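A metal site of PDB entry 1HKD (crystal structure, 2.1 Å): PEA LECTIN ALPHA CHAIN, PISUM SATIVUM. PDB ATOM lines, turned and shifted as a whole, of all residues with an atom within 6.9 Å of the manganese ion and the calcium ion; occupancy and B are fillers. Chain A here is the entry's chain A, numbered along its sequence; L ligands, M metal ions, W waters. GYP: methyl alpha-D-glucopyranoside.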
ATOM      1  N   ASP A  81     -27.065  14.448   4.520  1.00  0.00           N
ATOM      2  CA  ASP A  81     -26.051  13.782   5.332  1.00  0.00           C
ATOM      3  C   ASP A  81     -25.510  12.584   4.558  1.00  0.00           C
ATOM      4  O   ASP A  81     -24.404  12.095   4.767  1.00  0.00           O
ATOM      5  CB  ASP A  81     -26.728  13.243   6.570  1.00  0.00           C
ATOM      6  CG  ASP A  81     -26.739  14.242   7.662  1.00  0.00           C
ATOM      7  OD1 ASP A  81     -27.820  14.792   7.956  1.00  0.00           O
ATOM      8  OD2 ASP A  81     -25.701  14.567   8.257  1.00  0.00           O
ATOM      9  N   GLY A  82     -26.497  11.977   3.803  1.00  0.00           N
ATOM     10  CA  GLY A  82     -26.070  10.843   2.995  1.00  0.00           C
ATOM     11  C   GLY A  82     -27.182   9.859   2.730  1.00  0.00           C
ATOM     12  O   GLY A  82     -28.359  10.107   3.031  1.00  0.00           O
ATOM     13  N   GLY A  98     -30.576  12.804  10.651  1.00  0.00           N
ATOM     14  CA  GLY A  98     -29.340  13.550  10.536  1.00  0.00           C
ATOM     15  C   GLY A  98     -28.160  12.655  10.171  1.00  0.00           C
ATOM     16  O   GLY A  98     -28.264  11.793   9.284  1.00  0.00           O
ATOM     17  N   GLY A  99     -27.034  12.859  10.875  1.00  0.00           N
ATOM     18  CA  GLY A  99     -25.812  12.090  10.659  1.00  0.00           C
ATOM     19  C   GLY A  99     -25.933  10.587  10.946  1.00  0.00           C
ATOM     20  O   GLY A  99     -25.033   9.821  10.605  1.00  0.00           O
ATOM     21  N   TYR A 100     -27.029  10.192  11.590  1.00  0.00           N
ATOM     22  CA  TYR A 100     -27.277   8.792  11.892  1.00  0.00           C
ATOM     23  C   TYR A 100     -27.938   8.074  10.707  1.00  0.00           C
ATOM     24  O   TYR A 100     -28.198   6.872  10.760  1.00  0.00           O
ATOM     25  CB  TYR A 100     -28.123   8.655  13.172  1.00  0.00           C
ATOM     26  CG  TYR A 100     -27.384   9.104  14.410  1.00  0.00           C
ATOM     27  CD1 TYR A 100     -26.484   8.257  15.044  1.00  0.00           C
ATOM     28  CD2 TYR A 100     -27.509  10.403  14.882  1.00  0.00           C
ATOM     29  CE1 TYR A 100     -25.782   8.681  16.190  1.00  0.00           C
ATOM     30  CE2 TYR A 100     -26.825  10.832  15.998  1.00  0.00           C
ATOM     31  CZ  TYR A 100     -25.964   9.968  16.647  1.00  0.00           C
ATOM     32  OH  TYR A 100     -25.307  10.412  17.762  1.00  0.00           O
ATOM     33  N   LEU A 101     -28.245   8.841   9.664  1.00  0.00           N
ATOM     34  CA  LEU A 101     -28.771   8.306   8.390  1.00  0.00           C
ATOM     35  C   LEU A 101     -30.034   7.480   8.465  1.00  0.00           C
ATOM     36  O   LEU A 101     -30.309   6.690   7.546  1.00  0.00           O
ATOM     37  CB  LEU A 101     -27.676   7.534   7.642  1.00  0.00           C
ATOM     38  CG  LEU A 101     -26.332   8.273   7.542  1.00  0.00           C
ATOM     39  CD1 LEU A 101     -25.235   7.376   6.954  1.00  0.00           C
ATOM     40  CD2 LEU A 101     -26.485   9.552   6.721  1.00  0.00           C
ATOM     41  N   GLU A 119     -22.932   2.837   3.837  1.00  0.00           N
ATOM     42  CA  GLU A 119     -23.227   4.252   3.771  1.00  0.00           C
ATOM     43  C   GLU A 119     -22.443   4.991   2.704  1.00  0.00           C
ATOM     44  O   GLU A 119     -21.339   4.614   2.354  1.00  0.00           O
ATOM     45  CB  GLU A 119     -22.972   4.904   5.142  1.00  0.00           C
ATOM     46  CG  GLU A 119     -21.534   4.774   5.621  1.00  0.00           C
ATOM     47  CD  GLU A 119     -21.238   5.647   6.817  1.00  0.00           C
ATOM     48  OE1 GLU A 119     -20.262   6.411   6.767  1.00  0.00           O
ATOM     49  OE2 GLU A 119     -22.026   5.616   7.788  1.00  0.00           O
ATOM     50  N   PHE A 120     -23.053   6.064   2.204  1.00  0.00           N
ATOM     51  CA  PHE A 120     -22.428   6.984   1.260  1.00  0.00           C
ATOM     52  C   PHE A 120     -22.622   8.299   1.990  1.00  0.00           C
ATOM     53  O   PHE A 120     -23.674   8.928   1.898  1.00  0.00           O
ATOM     54  CB  PHE A 120     -23.163   6.932  -0.075  1.00  0.00           C
ATOM     55  CG  PHE A 120     -23.147   5.548  -0.709  1.00  0.00           C
ATOM     56  CD1 PHE A 120     -24.109   4.607  -0.360  1.00  0.00           C
ATOM     57  CD2 PHE A 120     -22.095   5.162  -1.523  1.00  0.00           C
ATOM     58  CE1 PHE A 120     -24.065   3.313  -0.871  1.00  0.00           C
ATOM     59  CE2 PHE A 120     -22.037   3.860  -2.037  1.00  0.00           C
ATOM     60  CZ  PHE A 120     -23.034   2.941  -1.717  1.00  0.00           C
ATOM     61  N   ASP A 121     -21.650   8.603   2.833  1.00  0.00           N
ATOM     62  CA  ASP A 121     -21.661   9.724   3.756  1.00  0.00           C
ATOM     63  C   ASP A 121     -21.104  11.018   3.158  1.00  0.00           C
ATOM     64  O   ASP A 121     -19.925  11.091   2.848  1.00  0.00           O
ATOM     65  CB  ASP A 121     -20.858   9.325   5.000  1.00  0.00           C
ATOM     66  CG  ASP A 121     -21.163  10.173   6.207  1.00  0.00           C
ATOM     67  OD1 ASP A 121     -21.611  11.343   6.057  1.00  0.00           O
ATOM     68  OD2 ASP A 121     -20.956   9.732   7.359  1.00  0.00           O
ATOM     69  N   THR A 122     -21.938  12.061   3.109  1.00  0.00           N
ATOM     70  CA  THR A 122     -21.516  13.330   2.519  1.00  0.00           C
ATOM     71  C   THR A 122     -21.175  14.428   3.519  1.00  0.00           C
ATOM     72  O   THR A 122     -20.794  15.533   3.108  1.00  0.00           O
ATOM     73  CB  THR A 122     -22.627  13.887   1.588  1.00  0.00           C
ATOM     74  OG1 THR A 122     -23.873  13.913   2.307  1.00  0.00           O
ATOM     75  CG2 THR A 122     -22.865  12.968   0.403  1.00  0.00           C
ATOM     76  N   PHE A 123     -21.377  14.166   4.803  1.00  0.00           N
ATOM     77  CA  PHE A 123     -21.131  15.186   5.818  1.00  0.00           C
ATOM     78  C   PHE A 123     -20.306  14.659   6.976  1.00  0.00           C
ATOM     79  O   PHE A 123     -20.668  13.670   7.609  1.00  0.00           O
ATOM     80  CB  PHE A 123     -22.474  15.768   6.325  1.00  0.00           C
ATOM     81  CG  PHE A 123     -22.331  16.847   7.365  1.00  0.00           C
ATOM     82  CD1 PHE A 123     -22.264  16.531   8.708  1.00  0.00           C
ATOM     83  CD2 PHE A 123     -22.331  18.194   6.999  1.00  0.00           C
ATOM     84  CE1 PHE A 123     -22.115  17.517   9.680  1.00  0.00           C
ATOM     85  CE2 PHE A 123     -22.197  19.195   7.962  1.00  0.00           C
ATOM     86  CZ  PHE A 123     -22.086  18.854   9.293  1.00  0.00           C
ATOM     87  N   TYR A 124     -19.213  15.364   7.254  1.00  0.00           N
ATOM     88  CA  TYR A 124     -18.304  15.032   8.336  1.00  0.00           C
ATOM     89  C   TYR A 124     -18.879  15.332   9.733  1.00  0.00           C
ATOM     90  O   TYR A 124     -19.031  16.495  10.107  1.00  0.00           O
ATOM     91  CB  TYR A 124     -16.976  15.801   8.156  1.00  0.00           C
ATOM     92  CG  TYR A 124     -16.032  15.723   9.347  1.00  0.00           C
ATOM     93  CD1 TYR A 124     -15.433  14.524   9.708  1.00  0.00           C
ATOM     94  CD2 TYR A 124     -15.767  16.856  10.126  1.00  0.00           C
ATOM     95  CE1 TYR A 124     -14.573  14.437  10.798  1.00  0.00           C
ATOM     96  CE2 TYR A 124     -14.894  16.787  11.226  1.00  0.00           C
ATOM     97  CZ  TYR A 124     -14.302  15.570  11.546  1.00  0.00           C
ATOM     98  OH  TYR A 124     -13.448  15.477  12.625  1.00  0.00           O
ATOM     99  N   ASN A 125     -19.178  14.277  10.494  1.00  0.00           N
ATOM    100  CA  ASN A 125     -19.632  14.404  11.873  1.00  0.00           C
ATOM    101  C   ASN A 125     -18.413  14.146  12.748  1.00  0.00           C
ATOM    102  O   ASN A 125     -17.930  13.017  12.809  1.00  0.00           O
ATOM    103  CB  ASN A 125     -20.730  13.385  12.181  1.00  0.00           C
ATOM    104  CG  ASN A 125     -22.021  13.650  11.434  1.00  0.00           C
ATOM    105  OD1 ASN A 125     -22.212  13.177  10.325  1.00  0.00           O
ATOM    106  ND2 ASN A 125     -22.936  14.383  12.066  1.00  0.00           N
ATOM    107  N   TRP A 128     -17.550  10.929  15.185  1.00  0.00           N
ATOM    108  CA  TRP A 128     -17.284   9.558  14.737  1.00  0.00           C
ATOM    109  C   TRP A 128     -16.719   9.358  13.317  1.00  0.00           C
ATOM    110  O   TRP A 128     -16.140   8.310  13.034  1.00  0.00           O
ATOM    111  CB  TRP A 128     -18.541   8.686  14.916  1.00  0.00           C
ATOM    112  CG  TRP A 128     -19.703   9.134  14.056  1.00  0.00           C
ATOM    113  CD1 TRP A 128     -19.817   8.999  12.705  1.00  0.00           C
ATOM    114  CD2 TRP A 128     -20.832   9.890  14.481  1.00  0.00           C
ATOM    115  NE1 TRP A 128     -20.986   9.587  12.260  1.00  0.00           N
ATOM    116  CE2 TRP A 128     -21.634  10.140  13.338  1.00  0.00           C
ATOM    117  CE3 TRP A 128     -21.292  10.347  15.714  1.00  0.00           C
ATOM    118  CZ2 TRP A 128     -22.831  10.842  13.396  1.00  0.00           C
ATOM    119  CZ3 TRP A 128     -22.486  11.040  15.775  1.00  0.00           C
ATOM    120  CH2 TRP A 128     -23.232  11.299  14.615  1.00  0.00           C
ATOM    121  N   ASP A 129     -16.869  10.345  12.432  1.00  0.00           N
ATOM    122  CA  ASP A 129     -16.381  10.183  11.053  1.00  0.00           C
ATOM    123  C   ASP A 129     -14.869  10.311  10.920  1.00  0.00           C
ATOM    124  O   ASP A 129     -14.222  10.941  11.756  1.00  0.00           O
ATOM    125  CB  ASP A 129     -17.080  11.175  10.133  1.00  0.00           C
ATOM    126  CG  ASP A 129     -18.472  10.726   9.735  1.00  0.00           C
ATOM    127  OD1 ASP A 129     -18.717   9.505   9.645  1.00  0.00           O
ATOM    128  OD2 ASP A 129     -19.372  11.554   9.446  1.00  0.00           O
ATOM    129  N   PRO A 130     -14.314   9.781   9.827  1.00  0.00           N
ATOM    130  CA  PRO A 130     -12.861   9.844   9.574  1.00  0.00           C
ATOM    131  C   PRO A 130     -12.335  11.271   9.724  1.00  0.00           C
ATOM    132  O   PRO A 130     -12.868  12.180   9.091  1.00  0.00           O
ATOM    133  CB  PRO A 130     -12.752   9.367   8.125  1.00  0.00           C
ATOM    134  CG  PRO A 130     -13.911   8.422   7.964  1.00  0.00           C
ATOM    135  CD  PRO A 130     -15.016   9.097   8.727  1.00  0.00           C
ATOM    136  N   HIS A 136     -17.221   9.890   2.233  1.00  0.00           N
ATOM    137  CA  HIS A 136     -16.712   8.529   2.166  1.00  0.00           C
ATOM    138  C   HIS A 136     -17.782   7.482   2.076  1.00  0.00           C
ATOM    139  O   HIS A 136     -18.947   7.724   2.383  1.00  0.00           O
ATOM    140  CB  HIS A 136     -15.897   8.257   3.440  1.00  0.00           C
ATOM    141  CG  HIS A 136     -16.621   8.617   4.706  1.00  0.00           C
ATOM    142  ND1 HIS A 136     -16.772   9.925   5.134  1.00  0.00           N
ATOM    143  CD2 HIS A 136     -17.323   7.851   5.588  1.00  0.00           C
ATOM    144  CE1 HIS A 136     -17.506   9.945   6.226  1.00  0.00           C
ATOM    145  NE2 HIS A 136     -17.857   8.704   6.524  1.00  0.00           N
ATOM    146  N   ILE A 137     -17.357   6.299   1.621  1.00  0.00           N
ATOM    147  CA  ILE A 137     -18.207   5.119   1.598  1.00  0.00           C
ATOM    148  C   ILE A 137     -17.813   4.351   2.855  1.00  0.00           C
ATOM    149  O   ILE A 137     -16.647   4.337   3.234  1.00  0.00           O
ATOM    150  CB  ILE A 137     -17.910   4.262   0.347  1.00  0.00           C
ATOM    151  CG1 ILE A 137     -18.154   5.077  -0.931  1.00  0.00           C
ATOM    152  CG2 ILE A 137     -18.788   3.008   0.326  1.00  0.00           C
ATOM    153  CD1 ILE A 137     -17.584   4.395  -2.192  1.00  0.00           C
ATOM    154  N   GLY A 138     -18.797   3.755   3.530  1.00  0.00           N
ATOM    155  CA  GLY A 138     -18.497   3.031   4.743  1.00  0.00           C
ATOM    156  C   GLY A 138     -19.356   1.806   4.949  1.00  0.00           C
ATOM    157  O   GLY A 138     -20.440   1.678   4.378  1.00  0.00           O
ATOM    158  N   ASP A 140     -21.175  -0.250   7.856  1.00  0.00           N
ATOM    159  CA  ASP A 140     -21.613  -0.044   9.227  1.00  0.00           C
ATOM    160  C   ASP A 140     -22.222  -1.304   9.809  1.00  0.00           C
ATOM    161  O   ASP A 140     -23.069  -1.945   9.175  1.00  0.00           O
ATOM    162  CB  ASP A 140     -22.636   1.098   9.284  1.00  0.00           C
ATOM    163  CG  ASP A 140     -22.087   2.424   8.772  1.00  0.00           C
ATOM    164  OD1 ASP A 140     -20.858   2.575   8.651  1.00  0.00           O
ATOM    165  OD2 ASP A 140     -22.842   3.385   8.489  1.00  0.00           O
ATOM    166  N   ILE A 144     -23.046   3.722  13.832  1.00  0.00           N
ATOM    167  CA  ILE A 144     -22.831   4.763  12.819  1.00  0.00           C
ATOM    168  C   ILE A 144     -21.336   4.962  12.539  1.00  0.00           C
ATOM    169  O   ILE A 144     -20.941   5.588  11.556  1.00  0.00           O
ATOM    170  CB  ILE A 144     -23.513   6.083  13.215  1.00  0.00           C
ATOM    171  CG1 ILE A 144     -23.652   7.019  12.000  1.00  0.00           C
ATOM    172  CG2 ILE A 144     -22.774   6.792  14.352  1.00  0.00           C
ATOM    173  CD1 ILE A 144     -24.458   6.415  10.842  1.00  0.00           C
ATOM    174  N   LYS A 145     -20.507   4.429  13.426  1.00  0.00           N
ATOM    175  CA  LYS A 145     -19.062   4.530  13.247  1.00  0.00           C
ATOM    176  C   LYS A 145     -18.616   3.300  12.463  1.00  0.00           C
ATOM    177  O   LYS A 145     -18.581   2.200  13.006  1.00  0.00           O
ATOM    178  CB  LYS A 145     -18.363   4.581  14.604  1.00  0.00           C
ATOM    179  CG  LYS A 145     -16.843   4.745  14.528  1.00  0.00           C
ATOM    180  CD  LYS A 145     -16.247   4.784  15.932  1.00  0.00           C
ATOM    181  CE  LYS A 145     -14.731   4.667  15.908  1.00  0.00           C
ATOM    182  NZ  LYS A 145     -14.140   4.730  17.292  1.00  0.00           N
ATOM    183  N   SER A 146     -18.284   3.502  11.185  1.00  0.00           N
ATOM    184  CA  SER A 146     -17.939   2.407  10.284  1.00  0.00           C
ATOM    185  C   SER A 146     -16.762   1.521  10.702  1.00  0.00           C
ATOM    186  O   SER A 146     -15.814   1.987  11.324  1.00  0.00           O
ATOM    187  CB  SER A 146     -17.694   2.950   8.864  1.00  0.00           C
ATOM    188  OG  SER A 146     -18.681   3.911   8.495  1.00  0.00           O
ATOM    189  N   THR A 149     -13.817   2.394   5.904  1.00  0.00           N
ATOM    190  CA  THR A 149     -14.281   3.460   5.026  1.00  0.00           C
ATOM    191  C   THR A 149     -13.334   3.646   3.851  1.00  0.00           C
ATOM    192  O   THR A 149     -12.201   3.140   3.855  1.00  0.00           O
ATOM    193  CB  THR A 149     -14.362   4.806   5.782  1.00  0.00           C
ATOM    194  OG1 THR A 149     -13.088   5.096   6.398  1.00  0.00           O
ATOM    195  CG2 THR A 149     -15.340   4.740   6.942  1.00  0.00           C
HETATM  196  C1  GYP L   1     -26.545  18.844  12.458  1.00  0.00           C
HETATM  197  C2  GYP L   1     -27.073  17.498  12.960  1.00  0.00           C
HETATM  198  C3  GYP L   1     -26.196  16.351  12.465  1.00  0.00           C
HETATM  199  C4  GYP L   1     -26.058  16.422  10.945  1.00  0.00           C
HETATM  200  C5  GYP L   1     -25.622  17.809  10.499  1.00  0.00           C
HETATM  201  C6  GYP L   1     -25.601  17.926   8.983  1.00  0.00           C
HETATM  202  C7  GYP L   1     -24.801  20.466  12.721  1.00  0.00           C
HETATM  203  O1  GYP L   1     -25.249  19.132  13.026  1.00  0.00           O
HETATM  204  O2  GYP L   1     -27.123  17.474  14.395  1.00  0.00           O
HETATM  205  O3  GYP L   1     -26.789  15.097  12.853  1.00  0.00           O
HETATM  206  O4  GYP L   1     -25.067  15.470  10.547  1.00  0.00           O
HETATM  207  O5  GYP L   1     -26.481  18.829  11.028  1.00  0.00           O
HETATM  208  O6  GYP L   1     -26.936  17.909   8.483  1.00  0.00           O
HETATM  209 MN    MN M   1     -19.492   8.092   8.110  1.00  0.00          MN
HETATM  210 CA    CA M   2     -21.607  11.806   8.509  1.00  0.00          CA
HETATM  211  O   HOH W   1     -21.167   7.302   9.529  1.00  0.00           O
HETATM  212  O   HOH W   2     -22.656   9.960   9.533  1.00  0.00           O
HETATM  213  O   HOH W   3     -18.169   6.460   8.900  1.00  0.00           O
HETATM  214  O   HOH W   4     -23.641  12.531   7.580  1.00  0.00           O
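Water W1 lies within hydrogen-bond range of the side-chain carboxylate of Glu 119 and the backbone carbonyl oxygen of Ile 144.
Water W2 bridges O of Gly 99 and NE1 of Trp 128.
The side-chain amide nitrogen (ND2) of Asn 125 is in hydrogen-bond range of an oxygen (O4) of the ligand (2.8 Å).
An oxygen (O3) of the ligand lies within hydrogen-bond range of the backbone NH of Gly 99 (3.0 Å).
OD2 of Asp 81 sits at hydrogen-bond distance from O4 of the ligand, at 2.5 Å.
Within 4 Å of the calcium ion: Asp 121, Phe 123, Asn 125 and Asp 129.
O of Phe 123 binds the calcium ion, at 2.3 Å.
The calcium ion is bound by water W4.
OD1 of Asn 125 is bound to the calcium ion (2.4 Å).
Water W2 binds the calcium ion.
The side-chain carboxylate (OD2) of Asp 129 binds the calcium ion (2.4 Å).
OD2 of Asp 121 binds the calcium ion (2.5 Å).
The side-chain carboxylate (OD1) of Asp 121 is bound to the calcium ion (2.5 Å).
O of Gly 138 sits at hydrogen-bond distance from N of Glu 119 (2.8 Å).
The side-chain carboxylate of Glu 119 lies close to the side-chain hydroxyl of Ser 146 (3.4 Å).
The side-chain carboxylate of Glu 119 sits close to the side-chain carboxylate of Asp 140.
The side-chain carboxylate (OD1) of Asp 129 sits close to the indole nitrogen (NE1) of Trp 128, 3.5 Å away.
Of the 24 residues printed, 4 come within 4 Å of the manganese ion.
The nearest printed residue that does not touch the manganese ion is Ser 146 (4.3 Å).
The manganese ion is bound by the side-chain carboxylate (OD1) of Asp 129 (2.2 Å), water W3 (2.2 Å), the side-chain carboxylate (OE1) of Glu 119 (2.3 Å), the side-chain carboxylate (OD2) of Asp 121 (2.3 Å), water W1 (2.3 Å) and a ring nitrogen (NE2) of His 136 (2.4 Å).
The manganese ion has six donor atoms within binding distance.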
